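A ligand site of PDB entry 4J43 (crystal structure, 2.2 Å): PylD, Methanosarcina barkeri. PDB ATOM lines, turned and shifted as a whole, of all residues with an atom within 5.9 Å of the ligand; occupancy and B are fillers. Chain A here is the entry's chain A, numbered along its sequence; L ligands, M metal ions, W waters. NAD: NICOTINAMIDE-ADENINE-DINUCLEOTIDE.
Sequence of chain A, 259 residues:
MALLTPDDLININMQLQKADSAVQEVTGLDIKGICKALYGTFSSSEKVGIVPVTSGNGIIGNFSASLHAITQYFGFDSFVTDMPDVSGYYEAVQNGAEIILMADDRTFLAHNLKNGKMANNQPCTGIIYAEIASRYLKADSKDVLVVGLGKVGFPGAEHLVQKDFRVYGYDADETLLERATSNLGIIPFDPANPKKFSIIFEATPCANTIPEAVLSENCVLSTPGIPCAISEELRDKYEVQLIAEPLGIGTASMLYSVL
ND2 of Asn 121 touches C5N of the ligand, 3.2 Å away.
Gln 122 touches the ligand (NE2 to O1N, 3.9 Å).
OG1 of Thr 125 touches C4N of the ligand (3.6 Å).
Val 147 touches the ligand (CG1 to C2A, 3.7 Å).
Gly 148 touches the ligand.
Gly 150 touches the ligand (CA to O5B, 3.4 Å).
Tyr 170 touches the ligand.
Asp 173 touches the ligand.
Leu 176 touches the ligand.
Ala 203 touches the ligand.
Pro 205 touches the ligand.
Thr 209 touches the ligand.
Gly 225 touches the ligand.
Leu 247 touches the ligand.
Hydrophobic or aromatic side chains within 4 Å of the ligand: Val 147, Val 152, Tyr 170, Ala 172, Leu 176, Pro 205 and Pro 224.
Within 4 Å of the ligand: Asn 121, Gln 122, Thr 125, Val 147, Gly 148, Gly 150, Lys 151, Val 152, Tyr 170, Asp 171, Ala 172, Asp 173, Leu 176, Ala 203, Thr 204, Pro 205, Cys 206, Thr 209, Pro 224, Gly 225, Ile 226, Glu 245, Pro 246 and Leu 247.
The side-chain carboxylate of Glu 245 sits at hydrogen-bond distance from the backbone NH of Leu 247 (3.1 Å).
The backbone carbonyl oxygen of Glu 245 sits at hydrogen-bond distance from the side-chain hydroxyl of Tyr 129, at 2.9 Å.
OE2 of Glu 245 is in hydrogen-bond range of N of Gly 248 (2.7 Å).
The backbone NH (N) of Ile 249 is in hydrogen-bond range of the side-chain carboxylate (OE2) of Glu 245, 2.8 Å away.
OG1 of Thr 125 is in hydrogen-bond range of O of Asn 121.
The backbone carbonyl oxygen (O) of Leu 247 sits at hydrogen-bond distance from the side-chain hydroxyl (OG1) of Thr 251, 2.9 Å away.
The backbone carbonyl oxygen of Val 147 lies within hydrogen-bond range of the backbone NH of Ala 203 (2.8 Å).
O of Tyr 170 is in hydrogen-bond range of N of Gly 148 (2.8 Å).
Water W1 lies within hydrogen-bond range of an oxygen (O2N) of the ligand, the backbone carbonyl oxygen (O) of Ala 203, the backbone NH (N) of Gly 150 and the backbone NH (N) of Gly 153.
Water W3 lies within hydrogen-bond range of O3B of the ligand (2.7 Å) and OD2 of Asp 173 (3.2 Å).
Water W6 lies within hydrogen-bond range of an oxygen (O1N) of the ligand and the side-chain amide nitrogen (NE2) of Gln 122.
Water W5 lies within hydrogen-bond range of O of Thr 209 (2.8 Å) and N1A of the ligand (2.9 Å).
An oxygen (O2B) of the ligand lies within hydrogen-bond range of the side-chain carboxylate (OD1) of Asp 171 (2.6 Å).
An oxygen (O2A) of the ligand lies within hydrogen-bond range of the backbone NH of Lys 151.
NZ of Lys 151 lies within salt-bridge range of O2A of the ligand, 2.8 Å away.
The backbone carbonyl oxygen (O) of Glu 245 lies within hydrogen-bond range of a nitrogen (N7N) of the ligand (2.8 Å).
The backbone NH (N) of Val 152 is in hydrogen-bond range of an oxygen (O2N) of the ligand, at 2.9 Å.
The side-chain hydroxyl (OG1) of Thr 204 is in hydrogen-bond range of an oxygen (O4B) of the ligand (3.0 Å).
The backbone carbonyl oxygen (O) of Pro 224 sits close to a nitrogen (N7N) of the ligand, 3.1 Å away.
O of Pro 246 lies close to N7N of the ligand, at 3.1 Å.
N3A of the ligand sits at hydrogen-bond distance from N of Ala 172.
The backbone NH (N) of Ile 226 is in hydrogen-bond range of an oxygen (O3D) of the ligand, 3.3 Å away.
O of Ile 226 lies within hydrogen-bond range of O3D of the ligand.
The side-chain sulfur (SG) of Cys 206 sits at hydrogen-bond distance from a nitrogen (N7A) of the ligand (3.6 Å).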
ATOM      1  N   ASN A 121      -6.315 -33.326 -17.796  1.00  0.00           N
ATOM      2  CA  ASN A 121      -6.516 -32.289 -18.809  1.00  0.00           C
ATOM      3  C   ASN A 121      -7.189 -31.018 -18.299  1.00  0.00           C
ATOM      4  O   ASN A 121      -6.838 -29.914 -18.742  1.00  0.00           O
ATOM      5  CB  ASN A 121      -7.329 -32.848 -19.993  1.00  0.00           C
ATOM      6  CG  ASN A 121      -7.560 -31.828 -21.094  1.00  0.00           C
ATOM      7  OD1 ASN A 121      -6.612 -31.358 -21.729  1.00  0.00           O
ATOM      8  ND2 ASN A 121      -8.815 -31.498 -21.330  1.00  0.00           N
ATOM      9  N   GLN A 122      -8.139 -31.160 -17.381  1.00  0.00           N
ATOM     10  CA  GLN A 122      -8.953 -30.028 -16.933  1.00  0.00           C
ATOM     11  C   GLN A 122      -8.168 -28.978 -16.118  1.00  0.00           C
ATOM     12  O   GLN A 122      -8.180 -27.801 -16.492  1.00  0.00           O
ATOM     13  CB  GLN A 122     -10.225 -30.500 -16.218  1.00  0.00           C
ATOM     14  CG  GLN A 122     -11.222 -31.144 -17.174  1.00  0.00           C
ATOM     15  CD  GLN A 122     -12.163 -32.128 -16.491  1.00  0.00           C
ATOM     16  OE1 GLN A 122     -11.920 -32.577 -15.368  1.00  0.00           O
ATOM     17  NE2 GLN A 122     -13.252 -32.458 -17.175  1.00  0.00           N
ATOM     18  N   THR A 125      -5.334 -27.514 -18.481  1.00  0.00           N
ATOM     19  CA  THR A 125      -5.868 -26.558 -19.455  1.00  0.00           C
ATOM     20  C   THR A 125      -6.139 -25.202 -18.803  1.00  0.00           C
ATOM     21  O   THR A 125      -5.720 -24.162 -19.313  1.00  0.00           O
ATOM     22  CB  THR A 125      -7.147 -27.094 -20.133  1.00  0.00           C
ATOM     23  OG1 THR A 125      -6.822 -28.278 -20.882  1.00  0.00           O
ATOM     24  CG2 THR A 125      -7.741 -26.070 -21.081  1.00  0.00           C
ATOM     25  N   TYR A 129      -3.974 -21.619 -19.748  1.00  0.00           N
ATOM     26  CA  TYR A 129      -4.701 -20.492 -20.324  1.00  0.00           C
ATOM     27  C   TYR A 129      -4.697 -19.280 -19.395  1.00  0.00           C
ATOM     28  O   TYR A 129      -4.619 -18.140 -19.851  1.00  0.00           O
ATOM     29  CB  TYR A 129      -6.139 -20.881 -20.707  1.00  0.00           C
ATOM     30  CG  TYR A 129      -6.262 -21.507 -22.089  1.00  0.00           C
ATOM     31  CD1 TYR A 129      -6.107 -22.879 -22.273  1.00  0.00           C
ATOM     32  CD2 TYR A 129      -6.566 -20.722 -23.201  1.00  0.00           C
ATOM     33  CE1 TYR A 129      -6.229 -23.456 -23.524  1.00  0.00           C
ATOM     34  CE2 TYR A 129      -6.700 -21.290 -24.468  1.00  0.00           C
ATOM     35  CZ  TYR A 129      -6.525 -22.652 -24.617  1.00  0.00           C
ATOM     36  OH  TYR A 129      -6.650 -23.231 -25.855  1.00  0.00           O
ATOM     37  N   VAL A 147     -14.407 -15.855 -15.965  1.00  0.00           N
ATOM     38  CA  VAL A 147     -15.786 -16.262 -16.172  1.00  0.00           C
ATOM     39  C   VAL A 147     -15.856 -17.784 -16.362  1.00  0.00           C
ATOM     40  O   VAL A 147     -15.341 -18.310 -17.349  1.00  0.00           O
ATOM     41  CB  VAL A 147     -16.446 -15.520 -17.360  1.00  0.00           C
ATOM     42  CG1 VAL A 147     -17.845 -16.036 -17.637  1.00  0.00           C
ATOM     43  CG2 VAL A 147     -16.486 -14.026 -17.086  1.00  0.00           C
ATOM     44  N   GLY A 148     -16.486 -18.456 -15.408  1.00  0.00           N
ATOM     45  CA  GLY A 148     -16.565 -19.908 -15.401  1.00  0.00           C
ATOM     46  C   GLY A 148     -15.587 -20.466 -14.386  1.00  0.00           C
ATOM     47  O   GLY A 148     -14.373 -20.354 -14.558  1.00  0.00           O
ATOM     48  N   LEU A 149     -16.129 -21.053 -13.323  1.00  0.00           N
ATOM     49  CA  LEU A 149     -15.300 -21.534 -12.211  1.00  0.00           C
ATOM     50  C   LEU A 149     -15.485 -23.038 -11.956  1.00  0.00           C
ATOM     51  O   LEU A 149     -15.472 -23.488 -10.814  1.00  0.00           O
ATOM     52  CB  LEU A 149     -15.576 -20.698 -10.953  1.00  0.00           C
ATOM     53  CG  LEU A 149     -15.203 -19.211 -11.020  1.00  0.00           C
ATOM     54  CD1 LEU A 149     -15.940 -18.402  -9.974  1.00  0.00           C
ATOM     55  CD2 LEU A 149     -13.696 -19.020 -10.882  1.00  0.00           C
ATOM     56  N   GLY A 150     -15.648 -23.793 -13.036  1.00  0.00           N
ATOM     57  CA  GLY A 150     -15.800 -25.254 -12.959  1.00  0.00           C
ATOM     58  C   GLY A 150     -14.460 -25.964 -12.954  1.00  0.00           C
ATOM     59  O   GLY A 150     -13.479 -25.467 -12.392  1.00  0.00           O
ATOM     60  N   LYS A 151     -14.411 -27.136 -13.582  1.00  0.00           N
ATOM     61  CA  LYS A 151     -13.222 -28.007 -13.549  1.00  0.00           C
ATOM     62  C   LYS A 151     -11.994 -27.394 -14.225  1.00  0.00           C
ATOM     63  O   LYS A 151     -10.857 -27.688 -13.841  1.00  0.00           O
ATOM     64  CB  LYS A 151     -13.520 -29.382 -14.165  1.00  0.00           C
ATOM     65  CG  LYS A 151     -14.685 -30.113 -13.530  1.00  0.00           C
ATOM     66  CD  LYS A 151     -14.957 -31.434 -14.235  1.00  0.00           C
ATOM     67  CE  LYS A 151     -16.441 -31.730 -14.303  1.00  0.00           C
ATOM     68  NZ  LYS A 151     -17.163 -30.822 -15.227  1.00  0.00           N
ATOM     69  N   VAL A 152     -12.226 -26.557 -15.228  1.00  0.00           N
ATOM     70  CA  VAL A 152     -11.146 -25.844 -15.926  1.00  0.00           C
ATOM     71  C   VAL A 152     -10.907 -24.462 -15.285  1.00  0.00           C
ATOM     72  O   VAL A 152      -9.767 -24.090 -15.028  1.00  0.00           O
ATOM     73  CB  VAL A 152     -11.437 -25.691 -17.433  1.00  0.00           C
ATOM     74  CG1 VAL A 152     -10.379 -24.850 -18.119  1.00  0.00           C
ATOM     75  CG2 VAL A 152     -11.533 -27.056 -18.110  1.00  0.00           C
ATOM     76  N   GLY A 153     -11.987 -23.735 -15.017  1.00  0.00           N
ATOM     77  CA  GLY A 153     -11.921 -22.358 -14.512  1.00  0.00           C
ATOM     78  C   GLY A 153     -11.323 -22.182 -13.125  1.00  0.00           C
ATOM     79  O   GLY A 153     -10.492 -21.297 -12.912  1.00  0.00           O
ATOM     80  N   TYR A 170     -16.695 -14.731 -11.870  1.00  0.00           N
ATOM     81  CA  TYR A 170     -18.129 -14.938 -12.032  1.00  0.00           C
ATOM     82  C   TYR A 170     -18.462 -16.326 -12.577  1.00  0.00           C
ATOM     83  O   TYR A 170     -17.768 -16.843 -13.453  1.00  0.00           O
ATOM     84  CB  TYR A 170     -18.759 -13.854 -12.921  1.00  0.00           C
ATOM     85  CG  TYR A 170     -20.260 -14.012 -13.075  1.00  0.00           C
ATOM     86  CD1 TYR A 170     -21.120 -13.726 -12.015  1.00  0.00           C
ATOM     87  CD2 TYR A 170     -20.816 -14.477 -14.260  1.00  0.00           C
ATOM     88  CE1 TYR A 170     -22.498 -13.887 -12.131  1.00  0.00           C
ATOM     89  CE2 TYR A 170     -22.194 -14.646 -14.398  1.00  0.00           C
ATOM     90  CZ  TYR A 170     -23.024 -14.345 -13.323  1.00  0.00           C
ATOM     91  OH  TYR A 170     -24.384 -14.503 -13.449  1.00  0.00           O
ATOM     92  N   ASP A 171     -19.522 -16.908 -12.023  1.00  0.00           N
ATOM     93  CA  ASP A 171     -20.098 -18.159 -12.519  1.00  0.00           C
ATOM     94  C   ASP A 171     -21.603 -18.079 -12.314  1.00  0.00           C
ATOM     95  O   ASP A 171     -22.062 -17.642 -11.256  1.00  0.00           O
ATOM     96  CB  ASP A 171     -19.516 -19.360 -11.764  1.00  0.00           C
ATOM     97  CG  ASP A 171     -19.820 -20.688 -12.448  1.00  0.00           C
ATOM     98  OD1 ASP A 171     -21.010 -21.065 -12.540  1.00  0.00           O
ATOM     99  OD2 ASP A 171     -18.870 -21.358 -12.894  1.00  0.00           O
ATOM    100  N   ALA A 172     -22.365 -18.494 -13.330  1.00  0.00           N
ATOM    101  CA  ALA A 172     -23.821 -18.471 -13.276  1.00  0.00           C
ATOM    102  C   ALA A 172     -24.390 -19.354 -12.156  1.00  0.00           C
ATOM    103  O   ALA A 172     -25.515 -19.153 -11.699  1.00  0.00           O
ATOM    104  CB  ALA A 172     -24.402 -18.872 -14.625  1.00  0.00           C
ATOM    105  N   ASP A 173     -23.595 -20.333 -11.722  1.00  0.00           N
ATOM    106  CA  ASP A 173     -23.928 -21.168 -10.577  1.00  0.00           C
ATOM    107  C   ASP A 173     -23.457 -20.462  -9.304  1.00  0.00           C
ATOM    108  O   ASP A 173     -22.246 -20.308  -9.092  1.00  0.00           O
ATOM    109  CB  ASP A 173     -23.282 -22.552 -10.722  1.00  0.00           C
ATOM    110  CG  ASP A 173     -23.625 -23.510  -9.582  1.00  0.00           C
ATOM    111  OD1 ASP A 173     -24.061 -23.061  -8.503  1.00  0.00           O
ATOM    112  OD2 ASP A 173     -23.452 -24.735  -9.778  1.00  0.00           O
ATOM    113  N   LEU A 176     -21.047 -22.444  -6.820  1.00  0.00           N
ATOM    114  CA  LEU A 176     -19.639 -22.459  -7.224  1.00  0.00           C
ATOM    115  C   LEU A 176     -18.964 -21.108  -7.045  1.00  0.00           C
ATOM    116  O   LEU A 176     -17.783 -21.044  -6.706  1.00  0.00           O
ATOM    117  CB  LEU A 176     -19.476 -22.959  -8.663  1.00  0.00           C
ATOM    118  CG  LEU A 176     -19.555 -24.465  -8.919  1.00  0.00           C
ATOM    119  CD1 LEU A 176     -19.407 -24.738 -10.410  1.00  0.00           C
ATOM    120  CD2 LEU A 176     -18.501 -25.231  -8.142  1.00  0.00           C
ATOM    121  N   ALA A 203     -13.781 -19.909 -19.078  1.00  0.00           N
ATOM    122  CA  ALA A 203     -13.776 -21.369 -19.151  1.00  0.00           C
ATOM    123  C   ALA A 203     -15.201 -21.887 -19.040  1.00  0.00           C
ATOM    124  O   ALA A 203     -15.620 -22.449 -18.021  1.00  0.00           O
ATOM    125  CB  ALA A 203     -12.881 -21.958 -18.069  1.00  0.00           C
ATOM    126  N   THR A 204     -15.956 -21.702 -20.126  1.00  0.00           N
ATOM    127  CA  THR A 204     -17.381 -21.951 -20.161  1.00  0.00           C
ATOM    128  C   THR A 204     -17.791 -22.567 -21.512  1.00  0.00           C
ATOM    129  O   THR A 204     -17.343 -22.088 -22.572  1.00  0.00           O
ATOM    130  CB  THR A 204     -18.146 -20.633 -19.867  1.00  0.00           C
ATOM    131  OG1 THR A 204     -18.281 -20.453 -18.444  1.00  0.00           O
ATOM    132  CG2 THR A 204     -19.504 -20.618 -20.486  1.00  0.00           C
ATOM    133  N   PRO A 205     -18.668 -23.607 -21.478  1.00  0.00           N
ATOM    134  CA  PRO A 205     -19.162 -24.251 -22.690  1.00  0.00           C
ATOM    135  C   PRO A 205     -20.256 -23.458 -23.405  1.00  0.00           C
ATOM    136  O   PRO A 205     -21.042 -24.023 -24.177  1.00  0.00           O
ATOM    137  CB  PRO A 205     -19.734 -25.574 -22.161  1.00  0.00           C
ATOM    138  CG  PRO A 205     -20.217 -25.223 -20.799  1.00  0.00           C
ATOM    139  CD  PRO A 205     -19.214 -24.240 -20.269  1.00  0.00           C
ATOM    140  N   CYS A 206     -20.297 -22.154 -23.165  1.00  0.00           N
ATOM    141  CA  CYS A 206     -21.356 -21.300 -23.712  1.00  0.00           C
ATOM    142  C   CYS A 206     -20.810 -20.119 -24.498  1.00  0.00           C
ATOM    143  O   CYS A 206     -19.642 -19.702 -24.332  1.00  0.00           O
ATOM    144  CB  CYS A 206     -22.282 -20.817 -22.588  1.00  0.00           C
ATOM    145  SG  CYS A 206     -22.981 -22.138 -21.583  1.00  0.00           S
ATOM    146  N   ALA A 207     -21.671 -19.587 -25.362  1.00  0.00           N
ATOM    147  CA  ALA A 207     -21.387 -18.398 -26.156  1.00  0.00           C
ATOM    148  C   ALA A 207     -21.883 -17.148 -25.439  1.00  0.00           C
ATOM    149  O   ALA A 207     -22.665 -17.234 -24.487  1.00  0.00           O
ATOM    150  CB  ALA A 207     -22.049 -18.515 -27.526  1.00  0.00           C
ATOM    151  N   ASN A 208     -21.402 -15.981 -25.884  1.00  0.00           N
ATOM    152  CA  ASN A 208     -21.845 -14.670 -25.381  1.00  0.00           C
ATOM    153  C   ASN A 208     -21.840 -14.548 -23.858  1.00  0.00           C
ATOM    154  O   ASN A 208     -22.817 -14.071 -23.261  1.00  0.00           O
ATOM    155  CB  ASN A 208     -23.218 -14.304 -25.970  1.00  0.00           C
ATOM    156  CG  ASN A 208     -23.237 -14.297 -27.486  1.00  0.00           C
ATOM    157  OD1 ASN A 208     -22.198 -14.268 -28.139  1.00  0.00           O
ATOM    158  ND2 ASN A 208     -24.444 -14.332 -28.059  1.00  0.00           N
ATOM    159  N   THR A 209     -20.748 -14.985 -23.240  1.00  0.00           N
ATOM    160  CA  THR A 209     -20.627 -14.959 -21.779  1.00  0.00           C
ATOM    161  C   THR A 209     -19.832 -13.731 -21.295  1.00  0.00           C
ATOM    162  O   THR A 209     -19.808 -13.451 -20.095  1.00  0.00           O
ATOM    163  CB  THR A 209     -19.963 -16.236 -21.244  1.00  0.00           C
ATOM    164  OG1 THR A 209     -18.663 -16.394 -21.828  1.00  0.00           O
ATOM    165  CG2 THR A 209     -20.815 -17.459 -21.572  1.00  0.00           C
ATOM    166  N   THR A 223      -9.275 -18.165 -23.608  1.00  0.00           N
ATOM    167  CA  THR A 223     -10.421 -19.055 -23.390  1.00  0.00           C
ATOM    168  C   THR A 223     -10.313 -20.427 -24.056  1.00  0.00           C
ATOM    169  O   THR A 223     -10.205 -20.519 -25.283  1.00  0.00           O
ATOM    170  CB  THR A 223     -11.774 -18.361 -23.756  1.00  0.00           C
ATOM    171  OG1 THR A 223     -12.853 -19.278 -23.557  1.00  0.00           O
ATOM    172  CG2 THR A 223     -11.777 -17.869 -25.203  1.00  0.00           C
ATOM    173  N   PRO A 224     -10.311 -21.497 -23.247  1.00  0.00           N
ATOM    174  CA  PRO A 224     -10.417 -22.847 -23.785  1.00  0.00           C
ATOM    175  C   PRO A 224     -11.873 -23.263 -24.037  1.00  0.00           C
ATOM    176  O   PRO A 224     -12.114 -24.300 -24.670  1.00  0.00           O
ATOM    177  CB  PRO A 224      -9.813 -23.712 -22.690  1.00  0.00           C
ATOM    178  CG  PRO A 224     -10.092 -22.959 -21.429  1.00  0.00           C
ATOM    179  CD  PRO A 224     -10.021 -21.502 -21.800  1.00  0.00           C
ATOM    180  N   GLY A 225     -12.814 -22.452 -23.563  1.00  0.00           N
ATOM    181  CA  GLY A 225     -14.242 -22.768 -23.644  1.00  0.00           C
ATOM    182  C   GLY A 225     -14.775 -22.889 -25.062  1.00  0.00           C
ATOM    183  O   GLY A 225     -14.328 -22.191 -25.969  1.00  0.00           O
ATOM    184  N   ILE A 226     -15.727 -23.797 -25.244  1.00  0.00           N
ATOM    185  CA  ILE A 226     -16.321 -24.072 -26.549  1.00  0.00           C
ATOM    186  C   ILE A 226     -17.858 -24.082 -26.407  1.00  0.00           C
ATOM    187  O   ILE A 226     -18.383 -24.844 -25.604  1.00  0.00           O
ATOM    188  CB  ILE A 226     -15.819 -25.426 -27.126  1.00  0.00           C
ATOM    189  CG1 ILE A 226     -14.287 -25.481 -27.133  1.00  0.00           C
ATOM    190  CG2 ILE A 226     -16.378 -25.645 -28.526  1.00  0.00           C
ATOM    191  CD1 ILE A 226     -13.707 -26.885 -27.199  1.00  0.00           C
ATOM    192  N   PRO A 227     -18.560 -23.237 -27.175  1.00  0.00           N
ATOM    193  CA  PRO A 227     -17.999 -22.291 -28.135  1.00  0.00           C
ATOM    194  C   PRO A 227     -17.497 -20.974 -27.508  1.00  0.00           C
ATOM    195  O   PRO A 227     -17.474 -20.811 -26.260  1.00  0.00           O
ATOM    196  CB  PRO A 227     -19.165 -22.025 -29.097  1.00  0.00           C
ATOM    197  CG  PRO A 227     -20.389 -22.215 -28.261  1.00  0.00           C
ATOM    198  CD  PRO A 227     -20.040 -23.249 -27.225  1.00  0.00           C
ATOM    199  N   GLU A 245      -8.042 -22.323 -28.716  1.00  0.00           N
ATOM    200  CA  GLU A 245      -7.634 -23.479 -29.496  1.00  0.00           C
ATOM    201  C   GLU A 245      -8.270 -24.733 -28.854  1.00  0.00           C
ATOM    202  O   GLU A 245      -8.331 -24.817 -27.620  1.00  0.00           O
ATOM    203  CB  GLU A 245      -6.092 -23.560 -29.534  1.00  0.00           C
ATOM    204  CG  GLU A 245      -5.513 -24.611 -30.462  1.00  0.00           C
ATOM    205  CD  GLU A 245      -5.462 -25.973 -29.813  1.00  0.00           C
ATOM    206  OE1 GLU A 245      -5.536 -26.991 -30.555  1.00  0.00           O
ATOM    207  OE2 GLU A 245      -5.366 -26.041 -28.574  1.00  0.00           O
ATOM    208  N   PRO A 246      -8.755 -25.670 -29.675  1.00  0.00           N
ATOM    209  CA  PRO A 246      -9.629 -26.721 -29.118  1.00  0.00           C
ATOM    210  C   PRO A 246      -8.985 -27.846 -28.298  1.00  0.00           C
ATOM    211  O   PRO A 246      -9.693 -28.503 -27.531  1.00  0.00           O
ATOM    212  CB  PRO A 246     -10.340 -27.298 -30.357  1.00  0.00           C
ATOM    213  CG  PRO A 246      -9.418 -27.007 -31.486  1.00  0.00           C
ATOM    214  CD  PRO A 246      -8.725 -25.710 -31.150  1.00  0.00           C
ATOM    215  N   LEU A 247      -7.668 -28.087 -28.438  1.00  0.00           N
ATOM    216  CA  LEU A 247      -7.061 -29.271 -27.807  1.00  0.00           C
ATOM    217  C   LEU A 247      -5.545 -29.212 -27.554  1.00  0.00           C
ATOM    218  O   LEU A 247      -5.072 -29.665 -26.509  1.00  0.00           O
ATOM    219  CB  LEU A 247      -7.411 -30.532 -28.629  1.00  0.00           C
ATOM    220  CG  LEU A 247      -7.051 -31.939 -28.121  1.00  0.00           C
ATOM    221  CD1 LEU A 247      -7.694 -32.255 -26.780  1.00  0.00           C
ATOM    222  CD2 LEU A 247      -7.466 -32.974 -29.166  1.00  0.00           C
ATOM    223  N   GLY A 248      -4.806 -28.673 -28.519  1.00  0.00           N
ATOM    224  CA  GLY A 248      -3.343 -28.661 -28.494  1.00  0.00           C
ATOM    225  C   GLY A 248      -2.670 -27.971 -27.328  1.00  0.00           C
ATOM    226  O   GLY A 248      -1.714 -28.498 -26.764  1.00  0.00           O
ATOM    227  N   ILE A 249      -3.154 -26.787 -26.952  1.00  0.00           N
ATOM    228  CA  ILE A 249      -2.541 -26.017 -25.867  1.00  0.00           C
ATOM    229  C   ILE A 249      -2.688 -26.758 -24.535  1.00  0.00           C
ATOM    230  O   ILE A 249      -1.718 -26.902 -23.793  1.00  0.00           O
ATOM    231  CB  ILE A 249      -3.082 -24.569 -25.780  1.00  0.00           C
ATOM    232  CG1 ILE A 249      -2.733 -23.808 -27.077  1.00  0.00           C
ATOM    233  CG2 ILE A 249      -2.520 -23.842 -24.566  1.00  0.00           C
ATOM    234  CD1 ILE A 249      -3.290 -22.396 -27.158  1.00  0.00           C
ATOM    235  N   GLY A 250      -3.889 -27.255 -24.260  1.00  0.00           N
ATOM    236  CA  GLY A 250      -4.157 -28.082 -23.087  1.00  0.00           C
ATOM    237  C   GLY A 250      -3.346 -29.376 -23.041  1.00  0.00           C
ATOM    238  O   GLY A 250      -2.892 -29.783 -21.972  1.00  0.00           O
ATOM    239  N   THR A 251      -3.158 -30.000 -24.208  1.00  0.00           N
ATOM    240  CA  THR A 251      -2.361 -31.231 -24.309  1.00  0.00           C
ATOM    241  C   THR A 251      -0.868 -30.976 -24.020  1.00  0.00           C
ATOM    242  O   THR A 251      -0.230 -31.755 -23.306  1.00  0.00           O
ATOM    243  CB  THR A 251      -2.556 -31.931 -25.679  1.00  0.00           C
ATOM    244  OG1 THR A 251      -3.940 -32.250 -25.861  1.00  0.00           O
ATOM    245  CG2 THR A 251      -1.744 -33.242 -25.767  1.00  0.00           C
HETATM  246  PA  NAD L   1     -17.697 -27.287 -16.202  1.00  0.00           P
HETATM  247  O1A NAD L   1     -19.143 -27.605 -16.498  1.00  0.00           O
HETATM  248  O2A NAD L   1     -16.963 -28.055 -15.133  1.00  0.00           O
HETATM  249  O5B NAD L   1     -17.557 -25.717 -15.867  1.00  0.00           O
HETATM  250  C5B NAD L   1     -18.223 -24.731 -16.660  1.00  0.00           C
HETATM  251  C4B NAD L   1     -18.785 -23.668 -15.720  1.00  0.00           C
HETATM  252  O4B NAD L   1     -19.197 -22.512 -16.454  1.00  0.00           O
HETATM  253  C3B NAD L   1     -20.005 -24.185 -14.979  1.00  0.00           C
HETATM  254  O3B NAD L   1     -19.739 -24.159 -13.577  1.00  0.00           O
HETATM  255  C2B NAD L   1     -21.126 -23.219 -15.320  1.00  0.00           C
HETATM  256  O2B NAD L   1     -21.903 -22.887 -14.172  1.00  0.00           O
HETATM  257  C1B NAD L   1     -20.379 -22.000 -15.843  1.00  0.00           C
HETATM  258  N9A NAD L   1     -21.167 -21.162 -16.782  1.00  0.00           N
HETATM  259  C8A NAD L   1     -21.951 -21.581 -17.795  1.00  0.00           C
HETATM  260  N7A NAD L   1     -22.520 -20.532 -18.437  1.00  0.00           N
HETATM  261  C5A NAD L   1     -22.087 -19.408 -17.835  1.00  0.00           C
HETATM  262  C6A NAD L   1     -22.291 -17.949 -17.991  1.00  0.00           C
HETATM  263  N6A NAD L   1     -23.095 -17.447 -18.964  1.00  0.00           N
HETATM  264  N1A NAD L   1     -21.649 -17.121 -17.140  1.00  0.00           N
HETATM  265  C2A NAD L   1     -20.852 -17.583 -16.163  1.00  0.00           C
HETATM  266  N3A NAD L   1     -20.615 -18.899 -15.959  1.00  0.00           N
HETATM  267  C4A NAD L   1     -21.197 -19.836 -16.740  1.00  0.00           C
HETATM  268  O3  NAD L   1     -16.907 -27.389 -17.600  1.00  0.00           O
HETATM  269  PN  NAD L   1     -15.302 -27.507 -17.666  1.00  0.00           P
HETATM  270  O1N NAD L   1     -14.919 -28.964 -17.531  1.00  0.00           O
HETATM  271  O2N NAD L   1     -14.701 -26.501 -16.719  1.00  0.00           O
HETATM  272  O5D NAD L   1     -14.983 -27.036 -19.168  1.00  0.00           O
HETATM  273  C5D NAD L   1     -15.231 -25.699 -19.604  1.00  0.00           C
HETATM  274  C4D NAD L   1     -15.101 -25.605 -21.122  1.00  0.00           C
HETATM  275  O4D NAD L   1     -13.742 -25.811 -21.540  1.00  0.00           O
HETATM  276  C3D NAD L   1     -15.928 -26.662 -21.838  1.00  0.00           C
HETATM  277  O3D NAD L   1     -16.522 -26.036 -22.985  1.00  0.00           O
HETATM  278  C2D NAD L   1     -14.913 -27.697 -22.298  1.00  0.00           C
HETATM  279  O2D NAD L   1     -15.370 -28.370 -23.462  1.00  0.00           O
HETATM  280  C1D NAD L   1     -13.699 -26.811 -22.561  1.00  0.00           C
HETATM  281  N1N NAD L   1     -12.384 -27.473 -22.577  1.00  0.00           N
HETATM  282  C2N NAD L   1     -11.529 -27.096 -23.555  1.00  0.00           C
HETATM  283  C3N NAD L   1     -10.253 -27.631 -23.678  1.00  0.00           C
HETATM  284  C7N NAD L   1      -9.350 -27.142 -24.784  1.00  0.00           C
HETATM  285  O7N NAD L   1      -8.257 -27.652 -24.954  1.00  0.00           O
HETATM  286  N7N NAD L   1      -9.762 -26.135 -25.552  1.00  0.00           N
HETATM  287  C4N NAD L   1      -9.846 -28.594 -22.751  1.00  0.00           C
HETATM  288  C5N NAD L   1     -10.741 -28.980 -21.746  1.00  0.00           C
HETATM  289  C6N NAD L   1     -12.012 -28.408 -21.676  1.00  0.00           C
HETATM  290 MG    MG M   1      -6.286 -26.223 -25.895  1.00  0.00          MG
HETATM  291  O   HOH W   1     -14.833 -23.953 -15.834  1.00  0.00           O
HETATM  292  O   HOH W   2     -24.565 -22.775 -15.315  1.00  0.00           O
HETATM  293  O   HOH W   3     -21.932 -25.403 -12.517  1.00  0.00           O
HETATM  294  O   HOH W   4      -6.866 -29.827 -24.097  1.00  0.00           O
HETATM  295  O   HOH W   5     -21.479 -14.360 -18.043  1.00  0.00           O
HETATM  296  O   HOH W   6     -13.790 -30.606 -19.564  1.00  0.00           O
